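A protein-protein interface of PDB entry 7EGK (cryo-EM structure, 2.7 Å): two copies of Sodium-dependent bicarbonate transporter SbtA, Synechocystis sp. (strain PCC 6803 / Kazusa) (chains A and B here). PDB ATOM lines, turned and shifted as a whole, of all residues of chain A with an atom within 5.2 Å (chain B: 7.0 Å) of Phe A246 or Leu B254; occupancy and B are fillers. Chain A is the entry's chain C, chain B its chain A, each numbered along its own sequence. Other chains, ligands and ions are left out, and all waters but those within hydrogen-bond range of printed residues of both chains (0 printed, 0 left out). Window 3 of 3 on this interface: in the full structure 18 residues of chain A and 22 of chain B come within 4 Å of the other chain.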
ATOM      1  N   MET A  49     -33.538   5.092   2.421  1.00  0.00           N
ATOM      2  CA  MET A  49     -32.127   5.079   2.790  1.00  0.00           C
ATOM      3  C   MET A  49     -31.272   5.815   1.769  1.00  0.00           C
ATOM      4  O   MET A  49     -30.276   6.447   2.131  1.00  0.00           O
ATOM      5  CB  MET A  49     -31.642   3.641   2.941  1.00  0.00           C
ATOM      6  CG  MET A  49     -31.974   3.006   4.267  1.00  0.00           C
ATOM      7  SD  MET A  49     -30.886   3.543   5.567  1.00  0.00           S
ATOM      8  CE  MET A  49     -29.337   2.878   4.982  1.00  0.00           C
ATOM      9  N   SER A 241     -21.611  11.237  12.300  1.00  0.00           N
ATOM     10  CA  SER A 241     -21.295   9.933  12.872  1.00  0.00           C
ATOM     11  C   SER A 241     -22.204   8.846  12.311  1.00  0.00           C
ATOM     12  O   SER A 241     -21.742   7.746  11.991  1.00  0.00           O
ATOM     13  CB  SER A 241     -21.390   9.992  14.393  1.00  0.00           C
ATOM     14  OG  SER A 241     -22.735  10.102  14.818  1.00  0.00           O
ATOM     15  N   VAL A 242     -23.501   9.132  12.179  1.00  0.00           N
ATOM     16  CA  VAL A 242     -24.409   8.140  11.616  1.00  0.00           C
ATOM     17  C   VAL A 242     -24.306   8.107  10.097  1.00  0.00           C
ATOM     18  O   VAL A 242     -24.687   7.114   9.471  1.00  0.00           O
ATOM     19  CB  VAL A 242     -25.855   8.407  12.092  1.00  0.00           C
ATOM     20  CG1 VAL A 242     -26.503   9.541  11.326  1.00  0.00           C
ATOM     21  CG2 VAL A 242     -26.697   7.152  12.026  1.00  0.00           C
ATOM     22  N   TYR A 243     -23.763   9.158   9.484  1.00  0.00           N
ATOM     23  CA  TYR A 243     -23.620   9.178   8.037  1.00  0.00           C
ATOM     24  C   TYR A 243     -22.457   8.302   7.593  1.00  0.00           C
ATOM     25  O   TYR A 243     -22.582   7.524   6.645  1.00  0.00           O
ATOM     26  CB  TYR A 243     -23.437  10.616   7.553  1.00  0.00           C
ATOM     27  CG  TYR A 243     -22.932  10.721   6.140  1.00  0.00           C
ATOM     28  CD1 TYR A 243     -23.768  10.466   5.067  1.00  0.00           C
ATOM     29  CD2 TYR A 243     -21.618  11.079   5.879  1.00  0.00           C
ATOM     30  CE1 TYR A 243     -23.305  10.551   3.778  1.00  0.00           C
ATOM     31  CE2 TYR A 243     -21.149  11.165   4.597  1.00  0.00           C
ATOM     32  CZ  TYR A 243     -21.994  10.905   3.551  1.00  0.00           C
ATOM     33  OH  TYR A 243     -21.506  10.993   2.272  1.00  0.00           O
ATOM     34  N   GLU A 244     -21.317   8.409   8.278  1.00  0.00           N
ATOM     35  CA  GLU A 244     -20.135   7.657   7.880  1.00  0.00           C
ATOM     36  C   GLU A 244     -20.236   6.189   8.258  1.00  0.00           C
ATOM     37  O   GLU A 244     -19.494   5.364   7.719  1.00  0.00           O
ATOM     38  CB  GLU A 244     -18.889   8.265   8.516  1.00  0.00           C
ATOM     39  CG  GLU A 244     -18.526   9.634   7.993  1.00  0.00           C
ATOM     40  CD  GLU A 244     -17.641  10.396   8.955  1.00  0.00           C
ATOM     41  OE1 GLU A 244     -17.463  11.618   8.769  1.00  0.00           O
ATOM     42  OE2 GLU A 244     -17.124   9.773   9.905  1.00  0.00           O
ATOM     43  N   GLY A 245     -21.127   5.844   9.178  1.00  0.00           N
ATOM     44  CA  GLY A 245     -21.237   4.476   9.633  1.00  0.00           C
ATOM     45  C   GLY A 245     -22.357   3.690   8.990  1.00  0.00           C
ATOM     46  O   GLY A 245     -22.245   2.473   8.828  1.00  0.00           O
ATOM     47  N   PHE A 246     -23.445   4.362   8.627  1.00  0.00           N
ATOM     48  CA  PHE A 246     -24.638   3.681   8.143  1.00  0.00           C
ATOM     49  C   PHE A 246     -25.036   4.075   6.731  1.00  0.00           C
ATOM     50  O   PHE A 246     -25.141   3.207   5.861  1.00  0.00           O
ATOM     51  CB  PHE A 246     -25.799   3.963   9.098  1.00  0.00           C
ATOM     52  CG  PHE A 246     -26.963   3.042   8.936  1.00  0.00           C
ATOM     53  CD1 PHE A 246     -26.804   1.678   9.046  1.00  0.00           C
ATOM     54  CD2 PHE A 246     -28.230   3.550   8.720  1.00  0.00           C
ATOM     55  CE1 PHE A 246     -27.881   0.835   8.920  1.00  0.00           C
ATOM     56  CE2 PHE A 246     -29.309   2.711   8.604  1.00  0.00           C
ATOM     57  CZ  PHE A 246     -29.135   1.354   8.697  1.00  0.00           C
ATOM     58  N   TYR A 247     -25.251   5.363   6.472  1.00  0.00           N
ATOM     59  CA  TYR A 247     -25.921   5.764   5.240  1.00  0.00           C
ATOM     60  C   TYR A 247     -24.969   5.774   4.055  1.00  0.00           C
ATOM     61  O   TYR A 247     -25.381   5.490   2.928  1.00  0.00           O
ATOM     62  CB  TYR A 247     -26.568   7.134   5.422  1.00  0.00           C
ATOM     63  CG  TYR A 247     -27.754   7.120   6.351  1.00  0.00           C
ATOM     64  CD1 TYR A 247     -29.019   6.819   5.883  1.00  0.00           C
ATOM     65  CD2 TYR A 247     -27.603   7.399   7.700  1.00  0.00           C
ATOM     66  CE1 TYR A 247     -30.101   6.804   6.731  1.00  0.00           C
ATOM     67  CE2 TYR A 247     -28.679   7.382   8.553  1.00  0.00           C
ATOM     68  CZ  TYR A 247     -29.923   7.083   8.064  1.00  0.00           C
ATOM     69  OH  TYR A 247     -31.001   7.063   8.912  1.00  0.00           O
ATOM     70  N   ASP A 248     -23.712   6.095   4.284  1.00  0.00           N
ATOM     71  CA  ASP A 248     -22.708   6.058   3.229  1.00  0.00           C
ATOM     72  C   ASP A 248     -22.173   4.660   2.892  1.00  0.00           C
ATOM     73  O   ASP A 248     -22.035   4.372   1.699  1.00  0.00           O
ATOM     74  CB  ASP A 248     -21.555   7.002   3.574  1.00  0.00           C
ATOM     75  CG  ASP A 248     -20.750   7.400   2.366  1.00  0.00           C
ATOM     76  OD1 ASP A 248     -21.231   7.194   1.235  1.00  0.00           O
ATOM     77  OD2 ASP A 248     -19.632   7.921   2.546  1.00  0.00           O
ATOM     78  N   PRO A 249     -21.841   3.760   3.841  1.00  0.00           N
ATOM     79  CA  PRO A 249     -21.346   2.444   3.397  1.00  0.00           C
ATOM     80  C   PRO A 249     -22.424   1.530   2.845  1.00  0.00           C
ATOM     81  O   PRO A 249     -22.093   0.524   2.209  1.00  0.00           O
ATOM     82  CB  PRO A 249     -20.719   1.854   4.667  1.00  0.00           C
ATOM     83  CG  PRO A 249     -20.510   2.986   5.549  1.00  0.00           C
ATOM     84  CD  PRO A 249     -21.662   3.865   5.302  1.00  0.00           C
ATOM     85  N   LEU A 250     -23.691   1.834   3.065  1.00  0.00           N
ATOM     86  CA  LEU A 250     -24.774   1.013   2.550  1.00  0.00           C
ATOM     87  C   LEU A 250     -25.385   1.565   1.273  1.00  0.00           C
ATOM     88  O   LEU A 250     -26.405   1.043   0.825  1.00  0.00           O
ATOM     89  CB  LEU A 250     -25.862   0.860   3.614  1.00  0.00           C
ATOM     90  CG  LEU A 250     -25.929  -0.424   4.439  1.00  0.00           C
ATOM     91  CD1 LEU A 250     -24.624  -0.707   5.141  1.00  0.00           C
ATOM     92  CD2 LEU A 250     -27.034  -0.281   5.458  1.00  0.00           C
ATOM     93  N   ILE B  42     -40.159  -3.506   8.698  1.00  0.00           N
ATOM     94  CA  ILE B  42     -38.874  -2.896   9.018  1.00  0.00           C
ATOM     95  C   ILE B  42     -38.809  -2.515  10.491  1.00  0.00           C
ATOM     96  O   ILE B  42     -37.752  -2.626  11.117  1.00  0.00           O
ATOM     97  CB  ILE B  42     -38.621  -1.685   8.102  1.00  0.00           C
ATOM     98  CG1 ILE B  42     -38.805  -2.080   6.641  1.00  0.00           C
ATOM     99  CG2 ILE B  42     -37.232  -1.112   8.304  1.00  0.00           C
ATOM    100  CD1 ILE B  42     -37.826  -3.124   6.166  1.00  0.00           C
ATOM    101  N   ILE B  45     -37.994  -5.759  12.586  1.00  0.00           N
ATOM    102  CA  ILE B  45     -36.636  -6.279  12.528  1.00  0.00           C
ATOM    103  C   ILE B  45     -35.639  -5.303  13.147  1.00  0.00           C
ATOM    104  O   ILE B  45     -34.536  -5.703  13.520  1.00  0.00           O
ATOM    105  CB  ILE B  45     -36.266  -6.649  11.078  1.00  0.00           C
ATOM    106  CG1 ILE B  45     -35.190  -7.733  11.052  1.00  0.00           C
ATOM    107  CG2 ILE B  45     -35.801  -5.442  10.286  1.00  0.00           C
ATOM    108  CD1 ILE B  45     -35.621  -9.032  11.657  1.00  0.00           C
ATOM    109  N   ILE B  46     -36.001  -4.029  13.300  1.00  0.00           N
ATOM    110  CA  ILE B  46     -35.085  -3.080  13.925  1.00  0.00           C
ATOM    111  C   ILE B  46     -35.055  -3.296  15.432  1.00  0.00           C
ATOM    112  O   ILE B  46     -33.983  -3.327  16.045  1.00  0.00           O
ATOM    113  CB  ILE B  46     -35.467  -1.635  13.548  1.00  0.00           C
ATOM    114  CG1 ILE B  46     -34.923  -1.295  12.166  1.00  0.00           C
ATOM    115  CG2 ILE B  46     -34.915  -0.628  14.537  1.00  0.00           C
ATOM    116  CD1 ILE B  46     -35.313   0.071  11.683  1.00  0.00           C
ATOM    117  N   VAL B  47     -36.228  -3.498  16.039  1.00  0.00           N
ATOM    118  CA  VAL B  47     -36.315  -3.773  17.472  1.00  0.00           C
ATOM    119  C   VAL B  47     -35.647  -5.105  17.802  1.00  0.00           C
ATOM    120  O   VAL B  47     -35.003  -5.250  18.849  1.00  0.00           O
ATOM    121  CB  VAL B  47     -37.788  -3.732  17.921  1.00  0.00           C
ATOM    122  CG1 VAL B  47     -37.944  -4.082  19.382  1.00  0.00           C
ATOM    123  CG2 VAL B  47     -38.366  -2.362  17.673  1.00  0.00           C
ATOM    124  N   MET B  49     -33.040  -6.275  16.100  1.00  0.00           N
ATOM    125  CA  MET B  49     -31.603  -6.100  15.922  1.00  0.00           C
ATOM    126  C   MET B  49     -30.986  -5.311  17.067  1.00  0.00           C
ATOM    127  O   MET B  49     -29.841  -5.566  17.453  1.00  0.00           O
ATOM    128  CB  MET B  49     -31.322  -5.404  14.594  1.00  0.00           C
ATOM    129  CG  MET B  49     -31.340  -6.317  13.394  1.00  0.00           C
ATOM    130  SD  MET B  49     -29.847  -7.271  13.245  1.00  0.00           S
ATOM    131  CE  MET B  49     -28.663  -5.967  12.959  1.00  0.00           C
ATOM    132  N   LEU B  50     -31.720  -4.344  17.615  1.00  0.00           N
ATOM    133  CA  LEU B  50     -31.185  -3.541  18.706  1.00  0.00           C
ATOM    134  C   LEU B  50     -31.173  -4.324  20.011  1.00  0.00           C
ATOM    135  O   LEU B  50     -30.218  -4.241  20.785  1.00  0.00           O
ATOM    136  CB  LEU B  50     -31.996  -2.256  18.862  1.00  0.00           C
ATOM    137  CG  LEU B  50     -32.052  -1.264  17.701  1.00  0.00           C
ATOM    138  CD1 LEU B  50     -32.656   0.035  18.151  1.00  0.00           C
ATOM    139  CD2 LEU B  50     -30.697  -1.026  17.100  1.00  0.00           C
ATOM    140  N   PHE B 246     -21.800  -7.680  12.548  1.00  0.00           N
ATOM    141  CA  PHE B 246     -23.173  -7.368  12.176  1.00  0.00           C
ATOM    142  C   PHE B 246     -23.905  -6.519  13.199  1.00  0.00           C
ATOM    143  O   PHE B 246     -24.396  -5.440  12.858  1.00  0.00           O
ATOM    144  CB  PHE B 246     -23.941  -8.673  11.952  1.00  0.00           C
ATOM    145  CG  PHE B 246     -25.228  -8.508  11.214  1.00  0.00           C
ATOM    146  CD1 PHE B 246     -25.255  -7.918   9.967  1.00  0.00           C
ATOM    147  CD2 PHE B 246     -26.409  -8.984  11.751  1.00  0.00           C
ATOM    148  CE1 PHE B 246     -26.439  -7.790   9.281  1.00  0.00           C
ATOM    149  CE2 PHE B 246     -27.589  -8.865  11.064  1.00  0.00           C
ATOM    150  CZ  PHE B 246     -27.607  -8.262   9.833  1.00  0.00           C
ATOM    151  N   TYR B 247     -23.986  -6.967  14.450  1.00  0.00           N
ATOM    152  CA  TYR B 247     -24.920  -6.360  15.391  1.00  0.00           C
ATOM    153  C   TYR B 247     -24.374  -5.070  15.979  1.00  0.00           C
ATOM    154  O   TYR B 247     -25.140  -4.148  16.273  1.00  0.00           O
ATOM    155  CB  TYR B 247     -25.266  -7.352  16.497  1.00  0.00           C
ATOM    156  CG  TYR B 247     -26.110  -8.508  16.025  1.00  0.00           C
ATOM    157  CD1 TYR B 247     -27.489  -8.408  15.978  1.00  0.00           C
ATOM    158  CD2 TYR B 247     -25.526  -9.697  15.618  1.00  0.00           C
ATOM    159  CE1 TYR B 247     -28.259  -9.461  15.545  1.00  0.00           C
ATOM    160  CE2 TYR B 247     -26.289 -10.751  15.183  1.00  0.00           C
ATOM    161  CZ  TYR B 247     -27.653 -10.628  15.147  1.00  0.00           C
ATOM    162  OH  TYR B 247     -28.421 -11.676  14.711  1.00  0.00           O
ATOM    163  N   PRO B 249     -21.799  -2.926  14.346  1.00  0.00           N
ATOM    164  CA  PRO B 249     -21.668  -1.794  13.413  1.00  0.00           C
ATOM    165  C   PRO B 249     -22.987  -1.279  12.870  1.00  0.00           C
ATOM    166  O   PRO B 249     -23.020  -0.184  12.299  1.00  0.00           O
ATOM    167  CB  PRO B 249     -20.791  -2.359  12.288  1.00  0.00           C
ATOM    168  CG  PRO B 249     -20.158  -3.536  12.854  1.00  0.00           C
ATOM    169  CD  PRO B 249     -21.181  -4.118  13.734  1.00  0.00           C
ATOM    170  N   LEU B 250     -24.071  -2.024  13.019  1.00  0.00           N
ATOM    171  CA  LEU B 250     -25.370  -1.584  12.540  1.00  0.00           C
ATOM    172  C   LEU B 250     -26.240  -0.989  13.635  1.00  0.00           C
ATOM    173  O   LEU B 250     -27.414  -0.722  13.386  1.00  0.00           O
ATOM    174  CB  LEU B 250     -26.105  -2.755  11.883  1.00  0.00           C
ATOM    175  CG  LEU B 250     -26.122  -2.869  10.360  1.00  0.00           C
ATOM    176  CD1 LEU B 250     -24.727  -2.881   9.783  1.00  0.00           C
ATOM    177  CD2 LEU B 250     -26.839  -4.144   9.983  1.00  0.00           C
ATOM    178  N   PHE B 251     -25.695  -0.760  14.830  1.00  0.00           N
ATOM    179  CA  PHE B 251     -26.523  -0.370  15.965  1.00  0.00           C
ATOM    180  C   PHE B 251     -26.962   1.084  15.868  1.00  0.00           C
ATOM    181  O   PHE B 251     -28.154   1.391  15.967  1.00  0.00           O
ATOM    182  CB  PHE B 251     -25.765  -0.610  17.267  1.00  0.00           C
ATOM    183  CG  PHE B 251     -26.609  -0.455  18.492  1.00  0.00           C
ATOM    184  CD1 PHE B 251     -27.575  -1.388  18.801  1.00  0.00           C
ATOM    185  CD2 PHE B 251     -26.443   0.628  19.331  1.00  0.00           C
ATOM    186  CE1 PHE B 251     -28.350  -1.254  19.931  1.00  0.00           C
ATOM    187  CE2 PHE B 251     -27.220   0.768  20.461  1.00  0.00           C
ATOM    188  CZ  PHE B 251     -28.172  -0.173  20.757  1.00  0.00           C
ATOM    189  N   ARG B 252     -26.006   2.000  15.687  1.00  0.00           N
ATOM    190  CA  ARG B 252     -26.317   3.425  15.744  1.00  0.00           C
ATOM    191  C   ARG B 252     -27.107   3.887  14.534  1.00  0.00           C
ATOM    192  O   ARG B 252     -27.833   4.881  14.618  1.00  0.00           O
ATOM    193  CB  ARG B 252     -25.040   4.248  15.859  1.00  0.00           C
ATOM    194  CG  ARG B 252     -24.313   4.064  17.156  1.00  0.00           C
ATOM    195  CD  ARG B 252     -23.073   4.918  17.219  1.00  0.00           C
ATOM    196  NE  ARG B 252     -22.357   4.723  18.473  1.00  0.00           N
ATOM    197  CZ  ARG B 252     -21.141   5.192  18.720  1.00  0.00           C
ATOM    198  NH1 ARG B 252     -20.494   5.886  17.793  1.00  0.00           N
ATOM    199  NH2 ARG B 252     -20.567   4.962  19.890  1.00  0.00           N
ATOM    200  N   GLY B 253     -26.983   3.195  13.414  1.00  0.00           N
ATOM    201  CA  GLY B 253     -27.735   3.569  12.243  1.00  0.00           C
ATOM    202  C   GLY B 253     -29.161   3.076  12.258  1.00  0.00           C
ATOM    203  O   GLY B 253     -30.069   3.779  11.813  1.00  0.00           O
ATOM    204  N   LEU B 254     -29.371   1.860  12.763  1.00  0.00           N
ATOM    205  CA  LEU B 254     -30.724   1.343  12.900  1.00  0.00           C
ATOM    206  C   LEU B 254     -31.478   2.052  14.012  1.00  0.00           C
ATOM    207  O   LEU B 254     -32.711   2.099  13.995  1.00  0.00           O
ATOM    208  CB  LEU B 254     -30.691  -0.159  13.161  1.00  0.00           C
ATOM    209  CG  LEU B 254     -30.362  -1.059  11.974  1.00  0.00           C
ATOM    210  CD1 LEU B 254     -30.224  -2.480  12.441  1.00  0.00           C
ATOM    211  CD2 LEU B 254     -31.411  -0.953  10.901  1.00  0.00           C
ATOM    212  N   LEU B 255     -30.759   2.611  14.982  1.00  0.00           N
ATOM    213  CA  LEU B 255     -31.407   3.359  16.049  1.00  0.00           C
ATOM    214  C   LEU B 255     -31.915   4.703  15.548  1.00  0.00           C
ATOM    215  O   LEU B 255     -32.941   5.200  16.024  1.00  0.00           O
ATOM    216  CB  LEU B 255     -30.435   3.535  17.211  1.00  0.00           C
ATOM    217  CG  LEU B 255     -30.869   4.361  18.412  1.00  0.00           C
ATOM    218  CD1 LEU B 255     -31.958   3.653  19.174  1.00  0.00           C
ATOM    219  CD2 LEU B 255     -29.684   4.590  19.282  1.00  0.00           C
ATOM    220  N   SER B 256     -31.230   5.293  14.569  1.00  0.00           N
ATOM    221  CA  SER B 256     -31.675   6.567  14.018  1.00  0.00           C
ATOM    222  C   SER B 256     -32.957   6.420  13.210  1.00  0.00           C
ATOM    223  O   SER B 256     -33.727   7.375  13.100  1.00  0.00           O
ATOM    224  CB  SER B 256     -30.574   7.179  13.158  1.00  0.00           C
ATOM    225  OG  SER B 256     -30.401   6.450  11.961  1.00  0.00           O
ATOM    226  N   ILE B 257     -33.206   5.243  12.640  1.00  0.00           N
ATOM    227  CA  ILE B 257     -34.487   5.005  11.988  1.00  0.00           C
ATOM    228  C   ILE B 257     -35.575   4.780  13.027  1.00  0.00           C
ATOM    229  O   ILE B 257     -36.704   5.254  12.869  1.00  0.00           O
ATOM    230  CB  ILE B 257     -34.375   3.827  11.002  1.00  0.00           C
ATOM    231  CG1 ILE B 257     -33.303   4.113   9.957  1.00  0.00           C
ATOM    232  CG2 ILE B 257     -35.694   3.562  10.305  1.00  0.00           C
ATOM    233  CD1 ILE B 257     -33.130   3.017   8.947  1.00  0.00           C
ATOM    234  N   LEU B 258     -35.251   4.079  14.118  1.00  0.00           N
ATOM    235  CA  LEU B 258     -36.222   3.882  15.189  1.00  0.00           C
ATOM    236  C   LEU B 258     -36.518   5.186  15.916  1.00  0.00           C
ATOM    237  O   LEU B 258     -37.641   5.400  16.381  1.00  0.00           O
ATOM    238  CB  LEU B 258     -35.721   2.828  16.171  1.00  0.00           C
ATOM    239  CG  LEU B 258     -36.747   2.359  17.202  1.00  0.00           C
ATOM    240  CD1 LEU B 258     -37.895   1.633  16.533  1.00  0.00           C
ATOM    241  CD2 LEU B 258     -36.107   1.497  18.254  1.00  0.00           C
ATOM    242  N   MET B 259     -35.527   6.075  16.010  1.00  0.00           N
ATOM    243  CA  MET B 259     -35.778   7.413  16.531  1.00  0.00           C
ATOM    244  C   MET B 259     -36.693   8.204  15.612  1.00  0.00           C
ATOM    245  O   MET B 259     -37.420   9.081  16.074  1.00  0.00           O
ATOM    246  CB  MET B 259     -34.469   8.171  16.718  1.00  0.00           C
ATOM    247  CG  MET B 259     -33.693   7.821  17.959  1.00  0.00           C
ATOM    248  SD  MET B 259     -34.623   8.099  19.460  1.00  0.00           S
ATOM    249  CE  MET B 259     -34.617   6.455  20.125  1.00  0.00           C
ATOM    250  N   ILE B 261     -39.134   6.729  13.839  1.00  0.00           N
ATOM    251  CA  ILE B 261     -40.441   6.102  14.034  1.00  0.00           C
ATOM    252  C   ILE B 261     -41.077   6.589  15.328  1.00  0.00           C
ATOM    253  O   ILE B 261     -42.224   7.047  15.348  1.00  0.00           O
ATOM    254  CB  ILE B 261     -40.307   4.571  14.025  1.00  0.00           C
ATOM    255  CG1 ILE B 261     -39.855   4.079  12.655  1.00  0.00           C
ATOM    256  CG2 ILE B 261     -41.609   3.916  14.424  1.00  0.00           C
ATOM    257  CD1 ILE B 261     -39.273   2.695  12.681  1.00  0.00           C
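5 positions are printed for both chains.
The side-chain hydroxyl (OG) of Ser B256 sits at hydrogen-bond distance from the backbone carbonyl oxygen (O) of Gly B253, 2.7 Å away.
Phe A246 touches three residues of chain B. Of the printed residues of chain A, Leu B254 touches Phe A246 (3.9 Å). No residue of chain B comes within 4 Å of Gly A245. Of the printed residues of chain B, Val A242 touches Arg B252, Gly B253 and Ser B256. Printed residues of chain A within 4 Å of Ser B256: Val A242 and Tyr A247. Printed residues of chain A within 4 Å of Gly B253: Val A242 (3.7 Å) and Phe A246 (3.4 Å). Printed residues of chain A within 4 Å of Ile B257: Phe A246 and Tyr A247. Leu B258 touches none of the printed residues of chain A. Met B49 touches none of the printed residues of chain A. The nearest printed residue of chain A that does not touch Leu B254 is Val A242 (6.0 Å).
Among the printed residues, pairs that only touch across the chains: Phe A246 with Gly B253 (3.4 Å), Val A242 with Arg B252 (3.6 Å), Val A242 with Gly B253 (3.7 Å), Val A242 with Ser B256 (3.8 Å), Phe A246 with Ile B257 (3.8 Å), Tyr A247 with Ile B257 (3.9 Å) and Phe A246 with Leu B254 (3.9 Å).
Printed residues of chain B that touch a printed residue of chain A: Arg B252, Gly B253, Leu B254, Ser B256 and Ile B257. Hydrophobic or aromatic side chains of chain B that line the printed part of chain A: Leu B254 and Ile B257. Hydrophobic or aromatic side chains of chain A that line the printed part of chain B: Val A242, Phe A246 and Tyr A247.
The side-chain hydroxyl (OG) of Ser B256 lies within hydrogen-bond range of the side-chain hydroxyl (OH) of Tyr A247.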
